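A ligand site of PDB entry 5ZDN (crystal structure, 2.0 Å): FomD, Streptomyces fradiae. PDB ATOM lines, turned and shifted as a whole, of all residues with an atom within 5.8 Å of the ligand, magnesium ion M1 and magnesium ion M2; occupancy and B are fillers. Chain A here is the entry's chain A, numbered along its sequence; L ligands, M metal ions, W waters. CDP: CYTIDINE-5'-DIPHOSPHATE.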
ATOM      1  N   LEU A  58     -18.334 -12.195  20.485  1.00  0.00           N
ATOM      2  CA  LEU A  58     -19.736 -12.489  20.335  1.00  0.00           C
ATOM      3  C   LEU A  58     -20.203 -11.835  19.087  1.00  0.00           C
ATOM      4  O   LEU A  58     -20.081 -10.607  18.931  1.00  0.00           O
ATOM      5  CB  LEU A  58     -20.511 -11.912  21.502  1.00  0.00           C
ATOM      6  CG  LEU A  58     -20.039 -12.202  22.912  1.00  0.00           C
ATOM      7  CD1 LEU A  58     -20.929 -11.485  23.905  1.00  0.00           C
ATOM      8  CD2 LEU A  58     -20.035 -13.654  23.217  1.00  0.00           C
ATOM      9  N   PHE A  60     -23.357 -10.789  16.842  1.00  0.00           N
ATOM     10  CA  PHE A  60     -24.790 -10.528  16.922  1.00  0.00           C
ATOM     11  C   PHE A  60     -25.402 -10.393  15.524  1.00  0.00           C
ATOM     12  O   PHE A  60     -24.801  -9.832  14.651  1.00  0.00           O
ATOM     13  CB  PHE A  60     -24.945  -9.219  17.713  1.00  0.00           C
ATOM     14  CG  PHE A  60     -24.487  -9.338  19.119  1.00  0.00           C
ATOM     15  CD1 PHE A  60     -25.252 -10.034  20.032  1.00  0.00           C
ATOM     16  CD2 PHE A  60     -23.307  -8.700  19.547  1.00  0.00           C
ATOM     17  CE1 PHE A  60     -24.815 -10.207  21.324  1.00  0.00           C
ATOM     18  CE2 PHE A  60     -22.855  -8.860  20.825  1.00  0.00           C
ATOM     19  CZ  PHE A  60     -23.620  -9.556  21.737  1.00  0.00           C
ATOM     20  N   PRO A  71     -29.844  -9.358  24.241  1.00  0.00           N
ATOM     21  CA  PRO A  71     -29.564  -8.680  25.492  1.00  0.00           C
ATOM     22  C   PRO A  71     -28.046  -8.578  25.804  1.00  0.00           C
ATOM     23  O   PRO A  71     -27.626  -7.581  26.400  1.00  0.00           O
ATOM     24  CB  PRO A  71     -30.402  -9.474  26.539  1.00  0.00           C
ATOM     25  CG  PRO A  71     -30.759 -10.831  25.891  1.00  0.00           C
ATOM     26  CD  PRO A  71     -30.647 -10.593  24.392  1.00  0.00           C
ATOM     27  N   TRP A  72     -27.204  -9.497  25.332  1.00  0.00           N
ATOM     28  CA  TRP A  72     -25.753  -9.347  25.667  1.00  0.00           C
ATOM     29  C   TRP A  72     -24.969  -8.222  25.013  1.00  0.00           C
ATOM     30  O   TRP A  72     -23.806  -7.963  25.436  1.00  0.00           O
ATOM     31  CB  TRP A  72     -25.026 -10.700  25.495  1.00  0.00           C
ATOM     32  CG  TRP A  72     -25.341 -11.722  26.521  1.00  0.00           C
ATOM     33  CD1 TRP A  72     -26.130 -11.597  27.618  1.00  0.00           C
ATOM     34  CD2 TRP A  72     -24.812 -13.050  26.565  1.00  0.00           C
ATOM     35  NE1 TRP A  72     -26.087 -12.760  28.354  1.00  0.00           N
ATOM     36  CE2 TRP A  72     -25.286 -13.661  27.730  1.00  0.00           C
ATOM     37  CE3 TRP A  72     -23.956 -13.754  25.739  1.00  0.00           C
ATOM     38  CZ2 TRP A  72     -24.994 -14.991  28.050  1.00  0.00           C
ATOM     39  CZ3 TRP A  72     -23.626 -15.068  26.093  1.00  0.00           C
ATOM     40  CH2 TRP A  72     -24.133 -15.649  27.223  1.00  0.00           C
ATOM     41  N   LEU A  74     -25.542  -5.169  25.595  1.00  0.00           N
ATOM     42  CA  LEU A  74     -25.232  -4.217  26.697  1.00  0.00           C
ATOM     43  C   LEU A  74     -23.744  -4.202  27.065  1.00  0.00           C
ATOM     44  O   LEU A  74     -23.087  -3.110  27.338  1.00  0.00           O
ATOM     45  CB  LEU A  74     -26.061  -4.572  27.895  1.00  0.00           C
ATOM     46  CG  LEU A  74     -25.776  -3.859  29.262  1.00  0.00           C
ATOM     47  CD1 LEU A  74     -26.171  -2.392  29.242  1.00  0.00           C
ATOM     48  CD2 LEU A  74     -26.572  -4.566  30.363  1.00  0.00           C
ATOM     49  N   PHE A  75     -23.189  -5.401  27.136  1.00  0.00           N
ATOM     50  CA  PHE A  75     -21.799  -5.603  27.495  1.00  0.00           C
ATOM     51  C   PHE A  75     -20.794  -5.441  26.322  1.00  0.00           C
ATOM     52  O   PHE A  75     -19.600  -5.528  26.519  1.00  0.00           O
ATOM     53  CB  PHE A  75     -21.627  -6.994  28.169  1.00  0.00           C
ATOM     54  CG  PHE A  75     -22.002  -7.045  29.628  1.00  0.00           C
ATOM     55  CD1 PHE A  75     -23.317  -7.219  30.005  1.00  0.00           C
ATOM     56  CD2 PHE A  75     -21.040  -6.910  30.619  1.00  0.00           C
ATOM     57  CE1 PHE A  75     -23.680  -7.314  31.303  1.00  0.00           C
ATOM     58  CE2 PHE A  75     -21.408  -7.025  31.962  1.00  0.00           C
ATOM     59  CZ  PHE A  75     -22.735  -7.201  32.304  1.00  0.00           C
ATOM     60  N   GLY A  76     -21.269  -5.230  25.098  1.00  0.00           N
ATOM     61  CA  GLY A  76     -20.408  -5.174  23.914  1.00  0.00           C
ATOM     62  C   GLY A  76     -20.187  -6.481  23.189  1.00  0.00           C
ATOM     63  O   GLY A  76     -20.991  -7.442  23.285  1.00  0.00           O
ATOM     64  N   ASP A  77     -19.096  -6.586  22.449  1.00  0.00           N
ATOM     65  CA  ASP A  77     -19.007  -7.744  21.541  1.00  0.00           C
ATOM     66  C   ASP A  77     -17.898  -8.747  21.948  1.00  0.00           C
ATOM     67  O   ASP A  77     -17.402  -9.599  21.141  1.00  0.00           O
ATOM     68  CB  ASP A  77     -19.004  -7.305  20.072  1.00  0.00           C
ATOM     69  CG  ASP A  77     -17.738  -6.635  19.677  1.00  0.00           C
ATOM     70  OD1 ASP A  77     -17.108  -5.993  20.551  1.00  0.00           O
ATOM     71  OD2 ASP A  77     -17.384  -6.724  18.473  1.00  0.00           O
ATOM     72  N   ARG A  78     -17.585  -8.729  23.231  1.00  0.00           N
ATOM     73  CA  ARG A  78     -16.825  -9.799  23.795  1.00  0.00           C
ATOM     74  C   ARG A  78     -17.408 -10.309  25.100  1.00  0.00           C
ATOM     75  O   ARG A  78     -18.057  -9.527  25.900  1.00  0.00           O
ATOM     76  CB  ARG A  78     -15.356  -9.402  23.900  1.00  0.00           C
ATOM     77  CG  ARG A  78     -15.076  -8.476  25.052  1.00  0.00           C
ATOM     78  CD  ARG A  78     -13.800  -7.646  24.872  1.00  0.00           C
ATOM     79  NE  ARG A  78     -12.561  -8.362  25.171  1.00  0.00           N
ATOM     80  CZ  ARG A  78     -12.113  -8.678  26.390  1.00  0.00           C
ATOM     81  NH1 ARG A  78     -12.819  -8.379  27.475  1.00  0.00           N
ATOM     82  NH2 ARG A  78     -10.936  -9.321  26.514  1.00  0.00           N
ATOM     83  N   TRP A  79     -17.104 -11.598  25.374  1.00  0.00           N
ATOM     84  CA  TRP A  79     -17.421 -12.254  26.661  1.00  0.00           C
ATOM     85  C   TRP A  79     -16.541 -11.666  27.721  1.00  0.00           C
ATOM     86  O   TRP A  79     -15.345 -11.977  27.752  1.00  0.00           O
ATOM     87  CB  TRP A  79     -17.179 -13.759  26.632  1.00  0.00           C
ATOM     88  CG  TRP A  79     -17.674 -14.439  27.907  1.00  0.00           C
ATOM     89  CD1 TRP A  79     -16.909 -15.067  28.810  1.00  0.00           C
ATOM     90  CD2 TRP A  79     -19.042 -14.500  28.405  1.00  0.00           C
ATOM     91  NE1 TRP A  79     -17.684 -15.528  29.847  1.00  0.00           N
ATOM     92  CE2 TRP A  79     -19.002 -15.190  29.613  1.00  0.00           C
ATOM     93  CE3 TRP A  79     -20.273 -14.020  27.936  1.00  0.00           C
ATOM     94  CZ2 TRP A  79     -20.193 -15.461  30.382  1.00  0.00           C
ATOM     95  CZ3 TRP A  79     -21.401 -14.200  28.688  1.00  0.00           C
ATOM     96  CH2 TRP A  79     -21.372 -14.981  29.899  1.00  0.00           C
ATOM     97  N   GLN A  80     -17.123 -10.788  28.539  1.00  0.00           N
ATOM     98  CA  GLN A  80     -16.390  -9.983  29.576  1.00  0.00           C
ATOM     99  C   GLN A  80     -16.096 -10.682  30.903  1.00  0.00           C
ATOM    100  O   GLN A  80     -15.108 -10.393  31.536  1.00  0.00           O
ATOM    101  CB  GLN A  80     -17.159  -8.700  29.899  1.00  0.00           C
ATOM    102  CG  GLN A  80     -17.536  -7.882  28.680  1.00  0.00           C
ATOM    103  CD  GLN A  80     -16.367  -7.229  28.011  1.00  0.00           C
ATOM    104  OE1 GLN A  80     -15.217  -7.448  28.342  1.00  0.00           O
ATOM    105  NE2 GLN A  80     -16.672  -6.347  27.084  1.00  0.00           N
ATOM    106  N   SER A  81     -16.930 -11.632  31.308  1.00  0.00           N
ATOM    107  CA  SER A  81     -16.753 -12.326  32.566  1.00  0.00           C
ATOM    108  C   SER A  81     -15.598 -13.380  32.517  1.00  0.00           C
ATOM    109  O   SER A  81     -14.822 -13.458  31.527  1.00  0.00           O
ATOM    110  CB  SER A  81     -18.072 -13.022  32.910  1.00  0.00           C
ATOM    111  OG  SER A  81     -18.216 -13.134  34.296  1.00  0.00           O
ATOM    112  N   ALA A  82     -15.455 -14.158  33.590  1.00  0.00           N
ATOM    113  CA  ALA A  82     -14.583 -15.350  33.531  1.00  0.00           C
ATOM    114  C   ALA A  82     -15.189 -16.369  32.548  1.00  0.00           C
ATOM    115  O   ALA A  82     -16.344 -16.282  32.202  1.00  0.00           O
ATOM    116  CB  ALA A  82     -14.432 -15.978  34.914  1.00  0.00           C
ATOM    117  N   TYR A 111     -25.551 -21.983  36.977  1.00  0.00           N
ATOM    118  CA  TYR A 111     -26.620 -21.327  36.244  1.00  0.00           C
ATOM    119  C   TYR A 111     -27.315 -22.260  35.200  1.00  0.00           C
ATOM    120  O   TYR A 111     -26.764 -22.551  34.141  1.00  0.00           O
ATOM    121  CB  TYR A 111     -26.017 -20.198  35.502  1.00  0.00           C
ATOM    122  CG  TYR A 111     -27.011 -19.221  34.944  1.00  0.00           C
ATOM    123  CD1 TYR A 111     -27.506 -19.332  33.651  1.00  0.00           C
ATOM    124  CD2 TYR A 111     -27.397 -18.140  35.680  1.00  0.00           C
ATOM    125  CE1 TYR A 111     -28.345 -18.337  33.132  1.00  0.00           C
ATOM    126  CE2 TYR A 111     -28.261 -17.189  35.172  1.00  0.00           C
ATOM    127  CZ  TYR A 111     -28.718 -17.312  33.900  1.00  0.00           C
ATOM    128  OH  TYR A 111     -29.572 -16.338  33.480  1.00  0.00           O
ATOM    129  N   GLU A 131     -35.737 -17.741  28.409  1.00  0.00           N
ATOM    130  CA  GLU A 131     -35.781 -16.710  29.543  1.00  0.00           C
ATOM    131  C   GLU A 131     -35.766 -17.301  30.902  1.00  0.00           C
ATOM    132  O   GLU A 131     -35.138 -16.753  31.779  1.00  0.00           O
ATOM    133  CB  GLU A 131     -36.948 -15.736  29.334  1.00  0.00           C
ATOM    134  CG  GLU A 131     -37.081 -14.746  30.449  1.00  0.00           C
ATOM    135  CD  GLU A 131     -35.908 -13.811  30.203  1.00  0.00           C
ATOM    136  OE1 GLU A 131     -34.802 -14.131  30.605  1.00  0.00           O
ATOM    137  OE2 GLU A 131     -36.051 -13.042  29.291  1.00  0.00           O
ATOM    138  N   ASP A 133     -34.579 -18.958  34.016  1.00  0.00           N
ATOM    139  CA  ASP A 133     -33.310 -19.433  34.612  1.00  0.00           C
ATOM    140  C   ASP A 133     -33.351 -19.890  36.101  1.00  0.00           C
ATOM    141  O   ASP A 133     -34.180 -19.406  36.877  1.00  0.00           O
ATOM    142  CB  ASP A 133     -32.219 -18.346  34.478  1.00  0.00           C
ATOM    143  CG  ASP A 133     -32.315 -17.568  33.201  1.00  0.00           C
ATOM    144  OD1 ASP A 133     -31.927 -18.078  32.090  1.00  0.00           O
ATOM    145  OD2 ASP A 133     -32.747 -16.335  33.282  1.00  0.00           O
ATOM    146  N   LYS A 146     -35.090 -17.348  38.494  1.00  0.00           N
ATOM    147  CA  LYS A 146     -34.759 -16.070  37.914  1.00  0.00           C
ATOM    148  C   LYS A 146     -35.595 -15.860  36.674  1.00  0.00           C
ATOM    149  O   LYS A 146     -35.737 -16.805  35.840  1.00  0.00           O
ATOM    150  CB  LYS A 146     -33.283 -16.071  37.558  1.00  0.00           C
ATOM    151  CG  LYS A 146     -32.851 -14.935  36.620  1.00  0.00           C
ATOM    152  CD  LYS A 146     -31.356 -14.646  36.781  1.00  0.00           C
ATOM    153  CE  LYS A 146     -30.794 -13.706  35.739  1.00  0.00           C
ATOM    154  NZ  LYS A 146     -30.944 -13.972  34.291  1.00  0.00           N
ATOM    155  N   ASP A 147     -36.098 -14.658  36.511  1.00  0.00           N
ATOM    156  CA  ASP A 147     -36.788 -14.247  35.303  1.00  0.00           C
ATOM    157  C   ASP A 147     -38.119 -15.025  35.036  1.00  0.00           C
ATOM    158  O   ASP A 147     -38.571 -15.055  33.905  1.00  0.00           O
ATOM    159  CB  ASP A 147     -35.930 -14.435  34.044  1.00  0.00           C
ATOM    160  CG  ASP A 147     -34.705 -13.487  33.998  1.00  0.00           C
ATOM    161  OD1 ASP A 147     -34.758 -12.482  34.689  1.00  0.00           O
ATOM    162  OD2 ASP A 147     -33.739 -13.734  33.234  1.00  0.00           O
ATOM    163  N   LYS A 150     -40.765 -12.183  34.126  1.00  0.00           N
ATOM    164  CA  LYS A 150     -40.273 -11.750  32.808  1.00  0.00           C
ATOM    165  C   LYS A 150     -40.687 -12.756  31.702  1.00  0.00           C
ATOM    166  O   LYS A 150     -41.289 -12.379  30.688  1.00  0.00           O
ATOM    167  CB  LYS A 150     -38.771 -11.582  32.805  1.00  0.00           C
ATOM    168  CG  LYS A 150     -38.195 -10.974  31.520  1.00  0.00           C
ATOM    169  CD  LYS A 150     -36.738 -10.649  31.758  1.00  0.00           C
ATOM    170  CE  LYS A 150     -35.933 -10.120  30.534  1.00  0.00           C
ATOM    171  NZ  LYS A 150     -34.608  -9.429  30.960  1.00  0.00           N
HETATM  172  O3B CDP L   1     -29.854 -12.115  32.515  1.00  0.00           O
HETATM  173  PB  CDP L   1     -29.180 -10.960  33.434  1.00  0.00           P
HETATM  174  O1B CDP L   1     -30.241  -9.982  33.617  1.00  0.00           O
HETATM  175  O2B CDP L   1     -28.524 -11.465  34.619  1.00  0.00           O
HETATM  176  O3A CDP L   1     -28.046 -10.244  32.590  1.00  0.00           O
HETATM  177  PA  CDP L   1     -27.275 -10.368  31.194  1.00  0.00           P
HETATM  178  O1A CDP L   1     -27.515  -9.213  30.286  1.00  0.00           O
HETATM  179  O2A CDP L   1     -27.669 -11.747  30.642  1.00  0.00           O
HETATM  180  O5' CDP L   1     -25.688 -10.551  31.510  1.00  0.00           O
HETATM  181  C5' CDP L   1     -25.482 -11.478  32.504  1.00  0.00           C
HETATM  182  C4' CDP L   1     -24.059 -11.788  32.698  1.00  0.00           C
HETATM  183  O4' CDP L   1     -23.444 -12.403  31.560  1.00  0.00           O
HETATM  184  C3' CDP L   1     -23.214 -10.554  32.971  1.00  0.00           C
HETATM  185  O3' CDP L   1     -23.389 -10.059  34.290  1.00  0.00           O
HETATM  186  C2' CDP L   1     -21.839 -11.115  32.662  1.00  0.00           C
HETATM  187  O2' CDP L   1     -21.496 -11.933  33.788  1.00  0.00           O
HETATM  188  C1' CDP L   1     -22.071 -12.083  31.464  1.00  0.00           C
HETATM  189  N1  CDP L   1     -21.798 -11.488  30.145  1.00  0.00           N
HETATM  190  C2  CDP L   1     -20.452 -11.287  29.784  1.00  0.00           C
HETATM  191  O2  CDP L   1     -19.593 -11.643  30.588  1.00  0.00           O
HETATM  192  N3  CDP L   1     -20.109 -10.691  28.650  1.00  0.00           N
HETATM  193  C4  CDP L   1     -21.128 -10.306  27.859  1.00  0.00           C
HETATM  194  N4  CDP L   1     -20.922  -9.705  26.721  1.00  0.00           N
HETATM  195  C5  CDP L   1     -22.432 -10.422  28.253  1.00  0.00           C
HETATM  196  C6  CDP L   1     -22.770 -11.038  29.400  1.00  0.00           C
HETATM  197 MG    MG M   1     -29.487 -13.025  30.728  1.00  0.00          MG
HETATM  198 MG    MG M   2     -32.143  -9.346  33.878  1.00  0.00          MG
HETATM  199 MG    MG M   3     -33.767 -15.219  31.813  1.00  0.00          MG
HETATM  200 MG    MG M   4     -31.606 -17.783  30.104  1.00  0.00          MG
HETATM  201  O   HOH W   1     -31.008 -14.181  31.205  1.00  0.00           O
HETATM  202  O   HOH W   2     -30.256  -8.910  30.058  1.00  0.00           O
HETATM  203  O   HOH W   3     -32.368 -10.102  35.585  1.00  0.00           O
HETATM  204  O   HOH W   4     -29.102 -13.692  28.721  1.00  0.00           O
HETATM  205  O   HOH W   5     -30.862 -11.335  29.884  1.00  0.00           O
HETATM  206  O   HOH W   6     -28.535 -10.338  36.989  1.00  0.00           O
HETATM  207  O   HOH W   7     -28.232 -14.271  31.069  1.00  0.00           O
HETATM  208  O   HOH W   8     -24.163 -11.488  36.750  1.00  0.00           O
HETATM  209  O   HOH W   9     -31.889  -8.498  31.963  1.00  0.00           O
HETATM  210  O   HOH W  10     -32.638 -11.083  33.055  1.00  0.00           O
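The side-chain amino group (NZ) of Lys 146 lies within salt-bridge range of an oxygen (O2B) of the ligand, at 3.5 Å.
NE1 of Trp 72 lies close to O2A of the ligand (3.0 Å).
N of Gln 80 is in hydrogen-bond range of N3 of the ligand (3.0 Å).
The backbone carbonyl oxygen of Arg 78 lies within hydrogen-bond range of a nitrogen (N4) of the ligand (3.0 Å).
The backbone NH (N) of Ser 81 lies within hydrogen-bond range of an oxygen (O2) of the ligand (2.8 Å).
NE1 of Trp 79 is in hydrogen-bond range of O of Ala 82.
OD2 of Asp 147 lies close to NZ of Lys 146 (3.0 Å).
NE2 of Gln 80 sits at hydrogen-bond distance from O of Phe 75, at 3.1 Å.
The backbone carbonyl oxygen (O) of Asp 133 is in hydrogen-bond range of the backbone NH (N) of Lys 146, 2.8 Å away.
The backbone NH of Leu 58 is in hydrogen-bond range of the backbone carbonyl oxygen of Asp 77 (2.8 Å).
The side-chain amino group (NZ) of Lys 146 sits at hydrogen-bond distance from the side-chain hydroxyl (OH) of Tyr 111 (2.9 Å).
NH1 of Arg 78 is in hydrogen-bond range of OE1 of Gln 80 (2.7 Å).
Leu 58 touches the ligand (CD1 to N4, 3.3 Å).
CB of Phe 75 touches N4 of the ligand, 3.2 Å away.
CZ3 of Trp 79 touches N1 of the ligand (3.1 Å).
Hydrophobic or aromatic side chains within 4 Å of the ligand: Leu 58, Trp 72, Phe 75 and Trp 79.
Within 4 Å of the ligand: Leu 58, Trp 72, Phe 75, Arg 78, Trp 79, Gln 80, Ser 81 and Lys 146.
Along chain A the residues within 4 Å of the ligand span positions 58 to 146.
The nearest printed residue that does not touch the ligand is Gly 76 (4.1 Å).
Merely in contact with magnesium ion M1: Lys 146 (3.96 Å).
Of the 19 residues printed, 1 comes within 4 Å of magnesium ion M1.
Merely in contact with magnesium ion M2: Lys 150 (3.8 Å).
Of the 19 residues printed, 1 comes within 4 Å of magnesium ion M2.
Magnesium ion M1 is bound by water W7, at 1.8 Å.
Magnesium ion M1 is bound by water W1, 2.0 Å away.
Magnesium ion M1 is bound by an oxygen (O3B) of the ligand, at 2.0 Å.
Water W4 binds magnesium ion M1 (2.1 Å).
O2A of the ligand is bound to magnesium ion M1 (2.2 Å).
Water W5 is bound to magnesium ion M1 (2.3 Å).
Magnesium ion M2 is bound by water W3 (1.9 Å), water W10 (2.0 Å), O1B of the ligand (2.0 Å) and water W9 (2.1 Å).
Magnesium ion M2 has four donor atoms within binding distance.
Water W1 lies within hydrogen-bond range of NZ of Lys 146 (3.1 Å) and OH of Tyr 111 (3.4 Å).
Water W10 lies within hydrogen-bond range of OD1 of Asp 147 (3.0 Å) and NZ of Lys 150 (3.3 Å).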
